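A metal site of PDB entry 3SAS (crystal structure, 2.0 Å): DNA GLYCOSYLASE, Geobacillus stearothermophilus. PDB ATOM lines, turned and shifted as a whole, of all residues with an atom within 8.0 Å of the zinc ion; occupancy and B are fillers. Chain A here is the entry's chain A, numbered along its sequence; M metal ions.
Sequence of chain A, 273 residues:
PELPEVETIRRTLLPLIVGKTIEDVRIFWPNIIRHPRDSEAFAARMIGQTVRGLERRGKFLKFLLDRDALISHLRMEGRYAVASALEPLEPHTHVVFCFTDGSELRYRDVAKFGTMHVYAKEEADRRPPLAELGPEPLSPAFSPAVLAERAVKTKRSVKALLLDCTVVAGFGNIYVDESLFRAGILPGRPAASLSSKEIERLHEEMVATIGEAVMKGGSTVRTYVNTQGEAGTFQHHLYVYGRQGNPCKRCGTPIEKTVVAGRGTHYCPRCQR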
ATOM      1  N   PHE A 181      23.628  11.396 -20.791  1.00  0.00           N
ATOM      2  CA  PHE A 181      24.146  11.658 -22.127  1.00  0.00           C
ATOM      3  C   PHE A 181      25.665  11.700 -22.122  1.00  0.00           C
ATOM      4  O   PHE A 181      26.319  11.096 -22.974  1.00  0.00           O
ATOM      5  CB  PHE A 181      23.616  12.943 -22.750  1.00  0.00           C
ATOM      6  CG  PHE A 181      24.364  13.320 -23.981  1.00  0.00           C
ATOM      7  CD1 PHE A 181      24.044  12.754 -25.215  1.00  0.00           C
ATOM      8  CD2 PHE A 181      25.444  14.176 -23.899  1.00  0.00           C
ATOM      9  CE1 PHE A 181      24.778  13.070 -26.346  1.00  0.00           C
ATOM     10  CE2 PHE A 181      26.186  14.503 -25.024  1.00  0.00           C
ATOM     11  CZ  PHE A 181      25.846  13.952 -26.262  1.00  0.00           C
ATOM     12  N   TYR A 239      22.987  19.396 -23.713  1.00  0.00           N
ATOM     13  CA  TYR A 239      23.236  18.442 -24.795  1.00  0.00           C
ATOM     14  C   TYR A 239      21.954  17.841 -25.313  1.00  0.00           C
ATOM     15  O   TYR A 239      21.781  17.677 -26.531  1.00  0.00           O
ATOM     16  CB  TYR A 239      24.145  17.317 -24.321  1.00  0.00           C
ATOM     17  CG  TYR A 239      25.558  17.755 -24.205  1.00  0.00           C
ATOM     18  CD1 TYR A 239      26.128  18.006 -22.957  1.00  0.00           C
ATOM     19  CD2 TYR A 239      26.336  17.960 -25.339  1.00  0.00           C
ATOM     20  CE1 TYR A 239      27.435  18.413 -22.858  1.00  0.00           C
ATOM     21  CE2 TYR A 239      27.647  18.375 -25.243  1.00  0.00           C
ATOM     22  CZ  TYR A 239      28.187  18.604 -23.986  1.00  0.00           C
ATOM     23  OH  TYR A 239      29.491  19.016 -23.874  1.00  0.00           O
ATOM     24  N   VAL A 240      21.065  17.491 -24.403  1.00  0.00           N
ATOM     25  CA  VAL A 240      19.878  16.753 -24.796  1.00  0.00           C
ATOM     26  C   VAL A 240      18.577  17.338 -24.264  1.00  0.00           C
ATOM     27  O   VAL A 240      17.549  17.308 -24.951  1.00  0.00           O
ATOM     28  CB  VAL A 240      19.957  15.260 -24.404  1.00  0.00           C
ATOM     29  CG1 VAL A 240      21.050  14.553 -25.237  1.00  0.00           C
ATOM     30  CG2 VAL A 240      20.216  15.118 -22.897  1.00  0.00           C
ATOM     31  N   PRO A 247      19.936  18.488 -33.746  1.00  0.00           N
ATOM     32  CA  PRO A 247      21.067  17.584 -33.914  1.00  0.00           C
ATOM     33  C   PRO A 247      21.880  17.500 -32.621  1.00  0.00           C
ATOM     34  O   PRO A 247      22.145  18.525 -32.001  1.00  0.00           O
ATOM     35  CB  PRO A 247      21.916  18.255 -35.002  1.00  0.00           C
ATOM     36  CG  PRO A 247      21.025  19.296 -35.610  1.00  0.00           C
ATOM     37  CD  PRO A 247      20.067  19.715 -34.553  1.00  0.00           C
ATOM     38  N   CYS A 248      22.258  16.277 -32.250  1.00  0.00           N
ATOM     39  CA  CYS A 248      23.206  16.050 -31.168  1.00  0.00           C
ATOM     40  C   CYS A 248      24.447  16.884 -31.403  1.00  0.00           C
ATOM     41  O   CYS A 248      24.945  16.975 -32.522  1.00  0.00           O
ATOM     42  CB  CYS A 248      23.587  14.577 -31.111  1.00  0.00           C
ATOM     43  SG  CYS A 248      24.824  14.205 -29.837  1.00  0.00           S
ATOM     44  N   LYS A 249      24.957  17.502 -30.343  1.00  0.00           N
ATOM     45  CA  LYS A 249      26.117  18.375 -30.436  1.00  0.00           C
ATOM     46  C   LYS A 249      27.424  17.597 -30.575  1.00  0.00           C
ATOM     47  O   LYS A 249      28.451  18.147 -30.950  1.00  0.00           O
ATOM     48  CB  LYS A 249      26.185  19.302 -29.212  1.00  0.00           C
ATOM     49  CG  LYS A 249      24.987  20.247 -29.074  1.00  0.00           C
ATOM     50  CD  LYS A 249      25.189  21.232 -27.924  1.00  0.00           C
ATOM     51  CE  LYS A 249      24.046  22.238 -27.851  1.00  0.00           C
ATOM     52  NZ  LYS A 249      24.112  23.117 -26.640  1.00  0.00           N
ATOM     53  N   ARG A 250      27.378  16.302 -30.278  1.00  0.00           N
ATOM     54  CA  ARG A 250      28.554  15.460 -30.483  1.00  0.00           C
ATOM     55  C   ARG A 250      28.550  14.597 -31.755  1.00  0.00           C
ATOM     56  O   ARG A 250      29.629  14.357 -32.321  1.00  0.00           O
ATOM     57  CB  ARG A 250      28.821  14.598 -29.248  1.00  0.00           C
ATOM     58  CG  ARG A 250      29.317  15.421 -28.080  1.00  0.00           C
ATOM     59  CD  ARG A 250      29.625  14.572 -26.871  1.00  0.00           C
ATOM     60  NE  ARG A 250      29.977  15.407 -25.718  1.00  0.00           N
ATOM     61  CZ  ARG A 250      30.260  14.937 -24.510  1.00  0.00           C
ATOM     62  NH1 ARG A 250      30.568  15.779 -23.531  1.00  0.00           N
ATOM     63  NH2 ARG A 250      30.224  13.635 -24.287  1.00  0.00           N
ATOM     64  N   CYS A 251      27.391  14.134 -32.216  1.00  0.00           N
ATOM     65  CA  CYS A 251      27.378  13.295 -33.429  1.00  0.00           C
ATOM     66  C   CYS A 251      26.426  13.754 -34.507  1.00  0.00           C
ATOM     67  O   CYS A 251      26.441  13.224 -35.621  1.00  0.00           O
ATOM     68  CB  CYS A 251      27.067  11.828 -33.081  1.00  0.00           C
ATOM     69  SG  CYS A 251      25.348  11.599 -32.579  1.00  0.00           S
ATOM     70  N   GLY A 252      25.578  14.731 -34.187  1.00  0.00           N
ATOM     71  CA  GLY A 252      24.646  15.256 -35.184  1.00  0.00           C
ATOM     72  C   GLY A 252      23.360  14.467 -35.361  1.00  0.00           C
ATOM     73  O   GLY A 252      22.440  14.900 -36.046  1.00  0.00           O
ATOM     74  N   THR A 253      23.280  13.292 -34.744  1.00  0.00           N
ATOM     75  CA  THR A 253      22.021  12.541 -34.724  1.00  0.00           C
ATOM     76  C   THR A 253      20.889  13.326 -34.046  1.00  0.00           C
ATOM     77  O   THR A 253      21.097  13.955 -33.006  1.00  0.00           O
ATOM     78  CB  THR A 253      22.228  11.219 -34.018  1.00  0.00           C
ATOM     79  OG1 THR A 253      23.296  10.511 -34.652  1.00  0.00           O
ATOM     80  CG2 THR A 253      20.943  10.382 -34.048  1.00  0.00           C
ATOM     81  N   PRO A 254      19.677  13.298 -34.619  1.00  0.00           N
ATOM     82  CA  PRO A 254      18.613  14.044 -33.937  1.00  0.00           C
ATOM     83  C   PRO A 254      18.333  13.551 -32.515  1.00  0.00           C
ATOM     84  O   PRO A 254      18.163  12.358 -32.274  1.00  0.00           O
ATOM     85  CB  PRO A 254      17.391  13.798 -34.834  1.00  0.00           C
ATOM     86  CG  PRO A 254      17.964  13.479 -36.194  1.00  0.00           C
ATOM     87  CD  PRO A 254      19.264  12.790 -35.952  1.00  0.00           C
ATOM     88  N   ILE A 255      18.286  14.481 -31.564  1.00  0.00           N
ATOM     89  CA  ILE A 255      17.917  14.137 -30.190  1.00  0.00           C
ATOM     90  C   ILE A 255      16.468  13.633 -30.146  1.00  0.00           C
ATOM     91  O   ILE A 255      15.595  14.173 -30.830  1.00  0.00           O
ATOM     92  CB  ILE A 255      18.130  15.334 -29.238  1.00  0.00           C
ATOM     93  CG1 ILE A 255      19.610  15.667 -29.185  1.00  0.00           C
ATOM     94  CG2 ILE A 255      17.569  15.056 -27.828  1.00  0.00           C
ATOM     95  CD1 ILE A 255      20.475  14.420 -29.069  1.00  0.00           C
ATOM     96  N   TYR A 267      17.444  12.085 -25.068  1.00  0.00           N
ATOM     97  CA  TYR A 267      18.663  11.317 -25.275  1.00  0.00           C
ATOM     98  C   TYR A 267      19.097  11.284 -26.741  1.00  0.00           C
ATOM     99  O   TYR A 267      18.301  11.562 -27.650  1.00  0.00           O
ATOM    100  CB  TYR A 267      18.451   9.893 -24.758  1.00  0.00           C
ATOM    101  CG  TYR A 267      17.388   9.160 -25.546  1.00  0.00           C
ATOM    102  CD1 TYR A 267      17.723   8.371 -26.649  1.00  0.00           C
ATOM    103  CD2 TYR A 267      16.039   9.275 -25.211  1.00  0.00           C
ATOM    104  CE1 TYR A 267      16.758   7.719 -27.380  1.00  0.00           C
ATOM    105  CE2 TYR A 267      15.058   8.615 -25.943  1.00  0.00           C
ATOM    106  CZ  TYR A 267      15.434   7.844 -27.026  1.00  0.00           C
ATOM    107  OH  TYR A 267      14.475   7.179 -27.758  1.00  0.00           O
ATOM    108  N   CYS A 268      20.364  10.936 -26.962  1.00  0.00           N
ATOM    109  CA  CYS A 268      20.874  10.664 -28.296  1.00  0.00           C
ATOM    110  C   CYS A 268      20.987   9.161 -28.478  1.00  0.00           C
ATOM    111  O   CYS A 268      21.722   8.492 -27.739  1.00  0.00           O
ATOM    112  CB  CYS A 268      22.247  11.299 -28.497  1.00  0.00           C
ATOM    113  SG  CYS A 268      22.946  10.867 -30.115  1.00  0.00           S
ATOM    114  N   PRO A 269      20.269   8.623 -29.473  1.00  0.00           N
ATOM    115  CA  PRO A 269      20.254   7.164 -29.662  1.00  0.00           C
ATOM    116  C   PRO A 269      21.560   6.662 -30.235  1.00  0.00           C
ATOM    117  O   PRO A 269      21.724   5.451 -30.351  1.00  0.00           O
ATOM    118  CB  PRO A 269      19.118   6.950 -30.682  1.00  0.00           C
ATOM    119  CG  PRO A 269      18.994   8.271 -31.388  1.00  0.00           C
ATOM    120  CD  PRO A 269      19.379   9.335 -30.401  1.00  0.00           C
ATOM    121  N   ARG A 270      22.462   7.560 -30.618  1.00  0.00           N
ATOM    122  CA  ARG A 270      23.746   7.107 -31.131  1.00  0.00           C
ATOM    123  C   ARG A 270      24.835   7.149 -30.075  1.00  0.00           C
ATOM    124  O   ARG A 270      25.575   6.184 -29.908  1.00  0.00           O
ATOM    125  CB  ARG A 270      24.178   7.878 -32.389  1.00  0.00           C
ATOM    126  CG  ARG A 270      25.535   7.435 -32.909  1.00  0.00           C
ATOM    127  CD  ARG A 270      25.961   8.180 -34.182  1.00  0.00           C
ATOM    128  NE  ARG A 270      27.209   7.609 -34.687  1.00  0.00           N
ATOM    129  CZ  ARG A 270      27.784   7.954 -35.827  1.00  0.00           C
ATOM    130  NH1 ARG A 270      28.916   7.360 -36.205  1.00  0.00           N
ATOM    131  NH2 ARG A 270      27.243   8.901 -36.589  1.00  0.00           N
ATOM    132  N   CYS A 271      24.942   8.282 -29.364  1.00  0.00           N
ATOM    133  CA  CYS A 271      25.933   8.411 -28.293  1.00  0.00           C
ATOM    134  C   CYS A 271      25.603   7.565 -27.077  1.00  0.00           C
ATOM    135  O   CYS A 271      26.506   7.123 -26.370  1.00  0.00           O
ATOM    136  CB  CYS A 271      26.101   9.885 -27.844  1.00  0.00           C
ATOM    137  SG  CYS A 271      26.798  10.973 -29.112  1.00  0.00           S
ATOM    138  N   GLN A 272      24.325   7.328 -26.819  1.00  0.00           N
ATOM    139  CA  GLN A 272      23.993   6.599 -25.613  1.00  0.00           C
ATOM    140  C   GLN A 272      23.657   5.139 -25.902  1.00  0.00           C
ATOM    141  O   GLN A 272      22.944   4.834 -26.851  1.00  0.00           O
ATOM    142  CB  GLN A 272      22.861   7.308 -24.840  1.00  0.00           C
ATOM    143  CG  GLN A 272      23.267   8.676 -24.317  1.00  0.00           C
ATOM    144  CD  GLN A 272      22.093   9.520 -23.883  1.00  0.00           C
ATOM    145  OE1 GLN A 272      21.694  10.450 -24.581  1.00  0.00           O
ATOM    146  NE2 GLN A 272      21.513   9.194 -22.720  1.00  0.00           N
HETATM  147 ZN    ZN M   1      25.027  11.889 -30.309  1.00  0.00          ZN
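Within 4 Å of the zinc ion: Cys 248, Cys 251, Cys 268 and Cys 271. The nearest printed residue that does not touch the zinc ion is Phe 181 (4.1 Å).
N of Cys 248 sits at hydrogen-bond distance from O of Thr 253, 2.7 Å away. The side-chain hydroxyl of Thr 253 lies close to the side-chain sulfur of Cys 251 (3.1 Å). SG of Cys 248 sits close to N of Arg 250, at 3.3 Å. The backbone NH (N) of Cys 268 sits at hydrogen-bond distance from the side-chain amide oxygen (OE1) of Gln 272, 2.8 Å away. SG of Cys 268 sits close to N of Arg 270, 3.4 Å away.
SG of Cys 251 is bound to the zinc ion (2.3 Å). The zinc ion is bound by SG of Cys 271, 2.3 Å away. The zinc ion is bound by SG of Cys 268 (2.3 Å). SG of Cys 248 is bound to the zinc ion, 2.4 Å away.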
